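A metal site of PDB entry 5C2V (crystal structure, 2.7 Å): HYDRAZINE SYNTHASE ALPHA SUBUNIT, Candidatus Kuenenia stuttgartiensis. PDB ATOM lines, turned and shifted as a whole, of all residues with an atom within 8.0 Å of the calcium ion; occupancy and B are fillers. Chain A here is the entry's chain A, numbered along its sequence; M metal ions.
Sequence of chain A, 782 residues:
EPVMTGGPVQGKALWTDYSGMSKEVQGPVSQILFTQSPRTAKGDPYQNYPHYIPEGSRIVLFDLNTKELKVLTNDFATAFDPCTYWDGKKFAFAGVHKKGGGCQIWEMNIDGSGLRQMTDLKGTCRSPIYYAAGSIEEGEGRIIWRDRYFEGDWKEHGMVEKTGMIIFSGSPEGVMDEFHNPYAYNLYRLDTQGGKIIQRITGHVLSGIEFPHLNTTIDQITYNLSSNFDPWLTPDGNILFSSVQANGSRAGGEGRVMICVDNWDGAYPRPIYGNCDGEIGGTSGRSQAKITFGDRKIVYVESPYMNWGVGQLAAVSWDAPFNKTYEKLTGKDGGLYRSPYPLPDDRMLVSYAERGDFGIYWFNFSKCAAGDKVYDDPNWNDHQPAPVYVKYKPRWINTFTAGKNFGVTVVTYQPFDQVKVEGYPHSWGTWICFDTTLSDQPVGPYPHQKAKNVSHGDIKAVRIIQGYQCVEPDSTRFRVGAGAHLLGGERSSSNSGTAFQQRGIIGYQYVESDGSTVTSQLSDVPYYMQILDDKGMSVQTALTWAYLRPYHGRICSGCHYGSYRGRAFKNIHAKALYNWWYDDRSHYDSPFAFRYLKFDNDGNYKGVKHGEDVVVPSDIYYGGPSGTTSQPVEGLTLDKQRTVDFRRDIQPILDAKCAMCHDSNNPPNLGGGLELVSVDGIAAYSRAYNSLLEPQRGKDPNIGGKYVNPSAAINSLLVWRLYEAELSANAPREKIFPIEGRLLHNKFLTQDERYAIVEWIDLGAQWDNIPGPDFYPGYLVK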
ATOM      1  N   PHE A  34      -8.188  15.528  17.934  1.00  0.00           N
ATOM      2  CA  PHE A  34      -8.726  16.693  18.652  1.00  0.00           C
ATOM      3  C   PHE A  34      -9.723  16.319  19.737  1.00  0.00           C
ATOM      4  O   PHE A  34     -10.244  15.206  19.776  1.00  0.00           O
ATOM      5  CB  PHE A  34      -9.355  17.695  17.672  1.00  0.00           C
ATOM      6  CG  PHE A  34     -10.593  17.197  16.993  1.00  0.00           C
ATOM      7  CD1 PHE A  34     -10.520  16.419  15.851  1.00  0.00           C
ATOM      8  CD2 PHE A  34     -11.845  17.523  17.486  1.00  0.00           C
ATOM      9  CE1 PHE A  34     -11.659  15.968  15.216  1.00  0.00           C
ATOM     10  CE2 PHE A  34     -12.996  17.079  16.861  1.00  0.00           C
ATOM     11  CZ  PHE A  34     -12.906  16.305  15.724  1.00  0.00           C
ATOM     12  N   GLN A  36     -13.242  16.680  21.803  1.00  0.00           N
ATOM     13  CA  GLN A  36     -14.649  17.038  21.767  1.00  0.00           C
ATOM     14  C   GLN A  36     -15.163  17.164  23.194  1.00  0.00           C
ATOM     15  O   GLN A  36     -15.031  16.233  24.000  1.00  0.00           O
ATOM     16  CB  GLN A  36     -15.461  15.996  20.999  1.00  0.00           C
ATOM     17  CG  GLN A  36     -15.176  15.967  19.512  1.00  0.00           C
ATOM     18  CD  GLN A  36     -16.070  14.999  18.763  1.00  0.00           C
ATOM     19  OE1 GLN A  36     -16.583  14.040  19.351  1.00  0.00           O
ATOM     20  NE2 GLN A  36     -16.270  15.242  17.469  1.00  0.00           N
ATOM     21  N   SER A  37     -15.741  18.312  23.512  1.00  0.00           N
ATOM     22  CA  SER A  37     -16.209  18.561  24.868  1.00  0.00           C
ATOM     23  C   SER A  37     -17.723  18.774  24.896  1.00  0.00           C
ATOM     24  O   SER A  37     -18.283  19.360  23.974  1.00  0.00           O
ATOM     25  CB  SER A  37     -15.499  19.783  25.462  1.00  0.00           C
ATOM     26  OG  SER A  37     -14.112  19.550  25.591  1.00  0.00           O
ATOM     27  N   ARG A  39     -21.162  20.495  25.659  1.00  0.00           N
ATOM     28  CA  ARG A  39     -21.353  21.930  25.710  1.00  0.00           C
ATOM     29  C   ARG A  39     -22.172  22.244  26.946  1.00  0.00           C
ATOM     30  O   ARG A  39     -23.388  22.096  26.988  1.00  0.00           O
ATOM     31  CB  ARG A  39     -22.056  22.412  24.436  1.00  0.00           C
ATOM     32  CG  ARG A  39     -21.542  21.704  23.199  1.00  0.00           C
ATOM     33  CD  ARG A  39     -22.390  22.069  22.005  1.00  0.00           C
ATOM     34  NE  ARG A  39     -22.713  23.485  22.014  1.00  0.00           N
ATOM     35  CZ  ARG A  39     -23.189  24.154  20.977  1.00  0.00           C
ATOM     36  NH1 ARG A  39     -23.416  23.528  19.830  1.00  0.00           N
ATOM     37  NH2 ARG A  39     -23.451  25.452  21.090  1.00  0.00           N
ATOM     38  N   SER A 351      -9.512  26.396  16.492  1.00  0.00           N
ATOM     39  CA  SER A 351     -10.852  26.047  16.926  1.00  0.00           C
ATOM     40  C   SER A 351     -11.714  27.299  16.982  1.00  0.00           C
ATOM     41  O   SER A 351     -11.463  28.191  17.780  1.00  0.00           O
ATOM     42  CB  SER A 351     -10.819  25.341  18.282  1.00  0.00           C
ATOM     43  OG  SER A 351     -12.131  25.064  18.746  1.00  0.00           O
ATOM     44  N   TYR A 352     -12.710  27.360  16.107  1.00  0.00           N
ATOM     45  CA  TYR A 352     -13.477  28.591  15.920  1.00  0.00           C
ATOM     46  C   TYR A 352     -14.966  28.410  16.162  1.00  0.00           C
ATOM     47  O   TYR A 352     -15.568  27.425  15.750  1.00  0.00           O
ATOM     48  CB  TYR A 352     -13.244  29.126  14.504  1.00  0.00           C
ATOM     49  CG  TYR A 352     -14.080  30.330  14.141  1.00  0.00           C
ATOM     50  CD1 TYR A 352     -13.922  31.536  14.808  1.00  0.00           C
ATOM     51  CD2 TYR A 352     -15.014  30.268  13.113  1.00  0.00           C
ATOM     52  CE1 TYR A 352     -14.685  32.644  14.469  1.00  0.00           C
ATOM     53  CE2 TYR A 352     -15.780  31.371  12.765  1.00  0.00           C
ATOM     54  CZ  TYR A 352     -15.606  32.558  13.454  1.00  0.00           C
ATOM     55  OH  TYR A 352     -16.362  33.659  13.118  1.00  0.00           O
ATOM     56  N   ALA A 353     -15.544  29.389  16.858  1.00  0.00           N
ATOM     57  CA  ALA A 353     -16.985  29.448  17.048  1.00  0.00           C
ATOM     58  C   ALA A 353     -17.520  30.750  16.469  1.00  0.00           C
ATOM     59  O   ALA A 353     -17.215  31.829  16.977  1.00  0.00           O
ATOM     60  CB  ALA A 353     -17.347  29.329  18.519  1.00  0.00           C
ATOM     61  N   GLY A 356     -21.100  30.937  18.942  1.00  0.00           N
ATOM     62  CA  GLY A 356     -21.221  30.070  20.089  1.00  0.00           C
ATOM     63  C   GLY A 356     -20.798  28.614  20.058  1.00  0.00           C
ATOM     64  O   GLY A 356     -20.771  27.991  21.099  1.00  0.00           O
ATOM     65  N   ASP A 357     -20.464  28.020  18.923  1.00  0.00           N
ATOM     66  CA  ASP A 357     -20.046  26.622  19.039  1.00  0.00           C
ATOM     67  C   ASP A 357     -18.861  26.282  18.152  1.00  0.00           C
ATOM     68  O   ASP A 357     -18.855  26.517  16.936  1.00  0.00           O
ATOM     69  CB  ASP A 357     -21.219  25.662  18.775  1.00  0.00           C
ATOM     70  CG  ASP A 357     -21.401  25.310  17.315  1.00  0.00           C
ATOM     71  OD1 ASP A 357     -21.454  26.231  16.471  1.00  0.00           O
ATOM     72  OD2 ASP A 357     -21.477  24.093  17.019  1.00  0.00           O
ATOM     73  N   PHE A 358     -17.844  25.736  18.798  1.00  0.00           N
ATOM     74  CA  PHE A 358     -16.508  25.609  18.246  1.00  0.00           C
ATOM     75  C   PHE A 358     -16.369  24.416  17.312  1.00  0.00           C
ATOM     76  O   PHE A 358     -17.030  23.394  17.484  1.00  0.00           O
ATOM     77  CB  PHE A 358     -15.488  25.515  19.373  1.00  0.00           C
ATOM     78  CG  PHE A 358     -15.351  26.775  20.181  1.00  0.00           C
ATOM     79  CD1 PHE A 358     -14.503  27.793  19.793  1.00  0.00           C
ATOM     80  CD2 PHE A 358     -16.124  26.956  21.312  1.00  0.00           C
ATOM     81  CE1 PHE A 358     -14.389  28.952  20.528  1.00  0.00           C
ATOM     82  CE2 PHE A 358     -16.030  28.117  22.063  1.00  0.00           C
ATOM     83  CZ  PHE A 358     -15.156  29.114  21.670  1.00  0.00           C
ATOM     84  N   GLY A 359     -15.499  24.560  16.317  1.00  0.00           N
ATOM     85  CA  GLY A 359     -15.168  23.478  15.420  1.00  0.00           C
ATOM     86  C   GLY A 359     -13.741  23.619  14.922  1.00  0.00           C
ATOM     87  O   GLY A 359     -13.091  24.629  15.169  1.00  0.00           O
ATOM     88  N   ILE A 360     -13.260  22.600  14.229  1.00  0.00           N
ATOM     89  CA  ILE A 360     -11.919  22.642  13.673  1.00  0.00           C
ATOM     90  C   ILE A 360     -11.952  23.312  12.303  1.00  0.00           C
ATOM     91  O   ILE A 360     -12.701  22.903  11.419  1.00  0.00           O
ATOM     92  CB  ILE A 360     -11.306  21.233  13.537  1.00  0.00           C
ATOM     93  CG1 ILE A 360     -11.504  20.462  14.848  1.00  0.00           C
ATOM     94  CG2 ILE A 360      -9.833  21.328  13.171  1.00  0.00           C
ATOM     95  CD1 ILE A 360     -10.894  21.136  16.054  1.00  0.00           C
ATOM     96  N   TYR A 361     -11.156  24.359  12.143  1.00  0.00           N
ATOM     97  CA  TYR A 361     -11.122  25.108  10.900  1.00  0.00           C
ATOM     98  C   TYR A 361      -9.697  25.430  10.477  1.00  0.00           C
ATOM     99  O   TYR A 361      -8.834  25.698  11.318  1.00  0.00           O
ATOM    100  CB  TYR A 361     -11.915  26.416  11.025  1.00  0.00           C
ATOM    101  CG  TYR A 361     -13.402  26.241  11.276  1.00  0.00           C
ATOM    102  CD1 TYR A 361     -13.891  26.045  12.559  1.00  0.00           C
ATOM    103  CD2 TYR A 361     -14.308  26.276  10.224  1.00  0.00           C
ATOM    104  CE1 TYR A 361     -15.242  25.884  12.792  1.00  0.00           C
ATOM    105  CE2 TYR A 361     -15.666  26.121  10.454  1.00  0.00           C
ATOM    106  CZ  TYR A 361     -16.125  25.927  11.741  1.00  0.00           C
ATOM    107  OH  TYR A 361     -17.476  25.765  11.974  1.00  0.00           O
ATOM    108  N   TYR A 375     -13.920  19.898  10.541  1.00  0.00           N
ATOM    109  CA  TYR A 375     -14.996  19.110  11.137  1.00  0.00           C
ATOM    110  C   TYR A 375     -15.745  19.893  12.207  1.00  0.00           C
ATOM    111  O   TYR A 375     -15.117  20.514  13.075  1.00  0.00           O
ATOM    112  CB  TYR A 375     -14.424  17.815  11.715  1.00  0.00           C
ATOM    113  CG  TYR A 375     -15.453  16.893  12.342  1.00  0.00           C
ATOM    114  CD1 TYR A 375     -16.138  15.965  11.564  1.00  0.00           C
ATOM    115  CD2 TYR A 375     -15.721  16.932  13.706  1.00  0.00           C
ATOM    116  CE1 TYR A 375     -17.074  15.114  12.132  1.00  0.00           C
ATOM    117  CE2 TYR A 375     -16.648  16.092  14.277  1.00  0.00           C
ATOM    118  CZ  TYR A 375     -17.326  15.180  13.486  1.00  0.00           C
ATOM    119  OH  TYR A 375     -18.255  14.334  14.048  1.00  0.00           O
ATOM    120  N   ASP A 376     -17.067  19.868  12.166  1.00  0.00           N
ATOM    121  CA  ASP A 376     -17.859  20.318  13.301  1.00  0.00           C
ATOM    122  C   ASP A 376     -19.075  19.443  13.546  1.00  0.00           C
ATOM    123  O   ASP A 376     -19.927  19.261  12.667  1.00  0.00           O
ATOM    124  CB  ASP A 376     -18.329  21.764  13.141  1.00  0.00           C
ATOM    125  CG  ASP A 376     -18.883  22.348  14.436  1.00  0.00           C
ATOM    126  OD1 ASP A 376     -19.989  21.959  14.876  1.00  0.00           O
ATOM    127  OD2 ASP A 376     -18.195  23.190  15.038  1.00  0.00           O
ATOM    128  N   ASP A 377     -19.160  18.915  14.761  1.00  0.00           N
ATOM    129  CA  ASP A 377     -20.392  18.343  15.259  1.00  0.00           C
ATOM    130  C   ASP A 377     -21.121  19.467  15.990  1.00  0.00           C
ATOM    131  O   ASP A 377     -20.475  20.267  16.668  1.00  0.00           O
ATOM    132  CB  ASP A 377     -20.119  17.157  16.181  1.00  0.00           C
ATOM    133  CG  ASP A 377     -21.361  16.343  16.489  1.00  0.00           C
ATOM    134  OD1 ASP A 377     -22.359  16.930  16.975  1.00  0.00           O
ATOM    135  OD2 ASP A 377     -21.347  15.116  16.265  1.00  0.00           O
ATOM    136  N   PRO A 378     -22.441  19.571  15.785  1.00  0.00           N
ATOM    137  CA  PRO A 378     -23.251  20.553  16.522  1.00  0.00           C
ATOM    138  C   PRO A 378     -23.416  20.191  18.001  1.00  0.00           C
ATOM    139  O   PRO A 378     -23.570  21.084  18.837  1.00  0.00           O
ATOM    140  CB  PRO A 378     -24.594  20.516  15.801  1.00  0.00           C
ATOM    141  CG  PRO A 378     -24.298  19.956  14.453  1.00  0.00           C
ATOM    142  CD  PRO A 378     -23.193  18.971  14.674  1.00  0.00           C
ATOM    143  N   ASN A 379     -23.377  18.906  18.318  1.00  0.00           N
ATOM    144  CA  ASN A 379     -23.603  18.446  19.681  1.00  0.00           C
ATOM    145  C   ASN A 379     -22.339  18.487  20.531  1.00  0.00           C
ATOM    146  O   ASN A 379     -22.392  18.280  21.752  1.00  0.00           O
ATOM    147  CB  ASN A 379     -24.172  17.025  19.684  1.00  0.00           C
ATOM    148  CG  ASN A 379     -25.554  16.945  19.064  1.00  0.00           C
ATOM    149  OD1 ASN A 379     -26.552  17.229  19.721  1.00  0.00           O
ATOM    150  ND2 ASN A 379     -25.614  16.561  17.795  1.00  0.00           N
ATOM    151  N   TRP A 380     -21.208  18.757  19.894  1.00  0.00           N
ATOM    152  CA  TRP A 380     -19.934  18.826  20.611  1.00  0.00           C
ATOM    153  C   TRP A 380     -19.209  20.136  20.360  1.00  0.00           C
ATOM    154  O   TRP A 380     -19.350  20.749  19.292  1.00  0.00           O
ATOM    155  CB  TRP A 380     -19.035  17.657  20.202  1.00  0.00           C
ATOM    156  CG  TRP A 380     -19.525  16.318  20.625  1.00  0.00           C
ATOM    157  CD1 TRP A 380     -20.258  15.442  19.873  1.00  0.00           C
ATOM    158  CD2 TRP A 380     -19.318  15.680  21.893  1.00  0.00           C
ATOM    159  NE1 TRP A 380     -20.530  14.309  20.595  1.00  0.00           N
ATOM    160  CE2 TRP A 380     -19.965  14.425  21.838  1.00  0.00           C
ATOM    161  CE3 TRP A 380     -18.663  16.053  23.060  1.00  0.00           C
ATOM    162  CZ2 TRP A 380     -19.969  13.544  22.915  1.00  0.00           C
ATOM    163  CZ3 TRP A 380     -18.667  15.172  24.138  1.00  0.00           C
ATOM    164  CH2 TRP A 380     -19.311  13.934  24.046  1.00  0.00           C
ATOM    165  N   ASN A 381     -18.439  20.566  21.349  1.00  0.00           N
ATOM    166  CA  ASN A 381     -17.510  21.678  21.161  1.00  0.00           C
ATOM    167  C   ASN A 381     -16.159  21.113  20.746  1.00  0.00           C
ATOM    168  O   ASN A 381     -15.490  20.428  21.524  1.00  0.00           O
ATOM    169  CB  ASN A 381     -17.389  22.509  22.442  1.00  0.00           C
ATOM    170  CG  ASN A 381     -17.902  23.930  22.259  1.00  0.00           C
ATOM    171  OD1 ASN A 381     -18.501  24.253  21.242  1.00  0.00           O
ATOM    172  ND2 ASN A 381     -17.646  24.775  23.250  1.00  0.00           N
ATOM    173  N   ASP A 382     -15.783  21.393  19.508  1.00  0.00           N
ATOM    174  CA  ASP A 382     -14.602  20.796  18.909  1.00  0.00           C
ATOM    175  C   ASP A 382     -13.394  21.724  19.014  1.00  0.00           C
ATOM    176  O   ASP A 382     -13.371  22.792  18.397  1.00  0.00           O
ATOM    177  CB  ASP A 382     -14.878  20.449  17.445  1.00  0.00           C
ATOM    178  CG  ASP A 382     -16.223  19.765  17.255  1.00  0.00           C
ATOM    179  OD1 ASP A 382     -16.479  18.759  17.949  1.00  0.00           O
ATOM    180  OD2 ASP A 382     -17.027  20.240  16.420  1.00  0.00           O
ATOM    181  N   HIS A 383     -12.409  21.326  19.801  1.00  0.00           N
ATOM    182  CA  HIS A 383     -11.230  22.163  20.012  1.00  0.00           C
ATOM    183  C   HIS A 383      -9.956  21.333  20.184  1.00  0.00           C
ATOM    184  O   HIS A 383      -9.980  20.115  20.074  1.00  0.00           O
ATOM    185  CB  HIS A 383     -11.427  23.061  21.239  1.00  0.00           C
ATOM    186  CG  HIS A 383     -11.611  22.323  22.523  1.00  0.00           C
ATOM    187  ND1 HIS A 383     -10.903  22.631  23.660  1.00  0.00           N
ATOM    188  CD2 HIS A 383     -12.433  21.297  22.861  1.00  0.00           C
ATOM    189  CE1 HIS A 383     -11.276  21.824  24.642  1.00  0.00           C
ATOM    190  NE2 HIS A 383     -12.200  21.004  24.170  1.00  0.00           N
HETATM  191 CA    CA M   1     -18.686  21.910  17.030  1.00  0.00          CA
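The backbone NH (N) of Phe 358 sits at hydrogen-bond distance from the side-chain amide oxygen (OD1) of Asn 381 (2.9 Å). The backbone NH (N) of Gly 359 lies close to the side-chain carboxylate (OD2) of Asp 376 (3.3 Å). N of Gly 359 sits at hydrogen-bond distance from O of Asp 382 (3.5 Å). The backbone carbonyl oxygen of Asp 382 sits at hydrogen-bond distance from the side-chain hydroxyl of Ser 351, 2.6 Å away. The side-chain carboxylate of Asp 377 is in hydrogen-bond range of the backbone NH of Asn 379. The side-chain carboxylate of Asp 357 lies within salt-bridge range of the guanidinium group of Arg 39 (3.5 Å).
Asp 357 touches the calcium ion (OD2 to CA, 3.5 Å). Six residues have an atom within 4 Å of the calcium ion: Asp 357, Phe 358, Asp 376, Asp 377, Trp 380 and Asp 382.
O of Phe 358 binds the calcium ion (2.3 Å). The side-chain carboxylate (OD2) of Asp 376 binds the calcium ion (2.4 Å). OD2 of Asp 382 is bound to the calcium ion. The backbone carbonyl oxygen (O) of Asp 377 binds the calcium ion (2.5 Å). The calcium ion is bound by OD1 of Asp 376 (2.5 Å). The backbone carbonyl oxygen (O) of Trp 380 is bound to the calcium ion (2.6 Å). The calcium ion has six donor atoms within binding distance.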
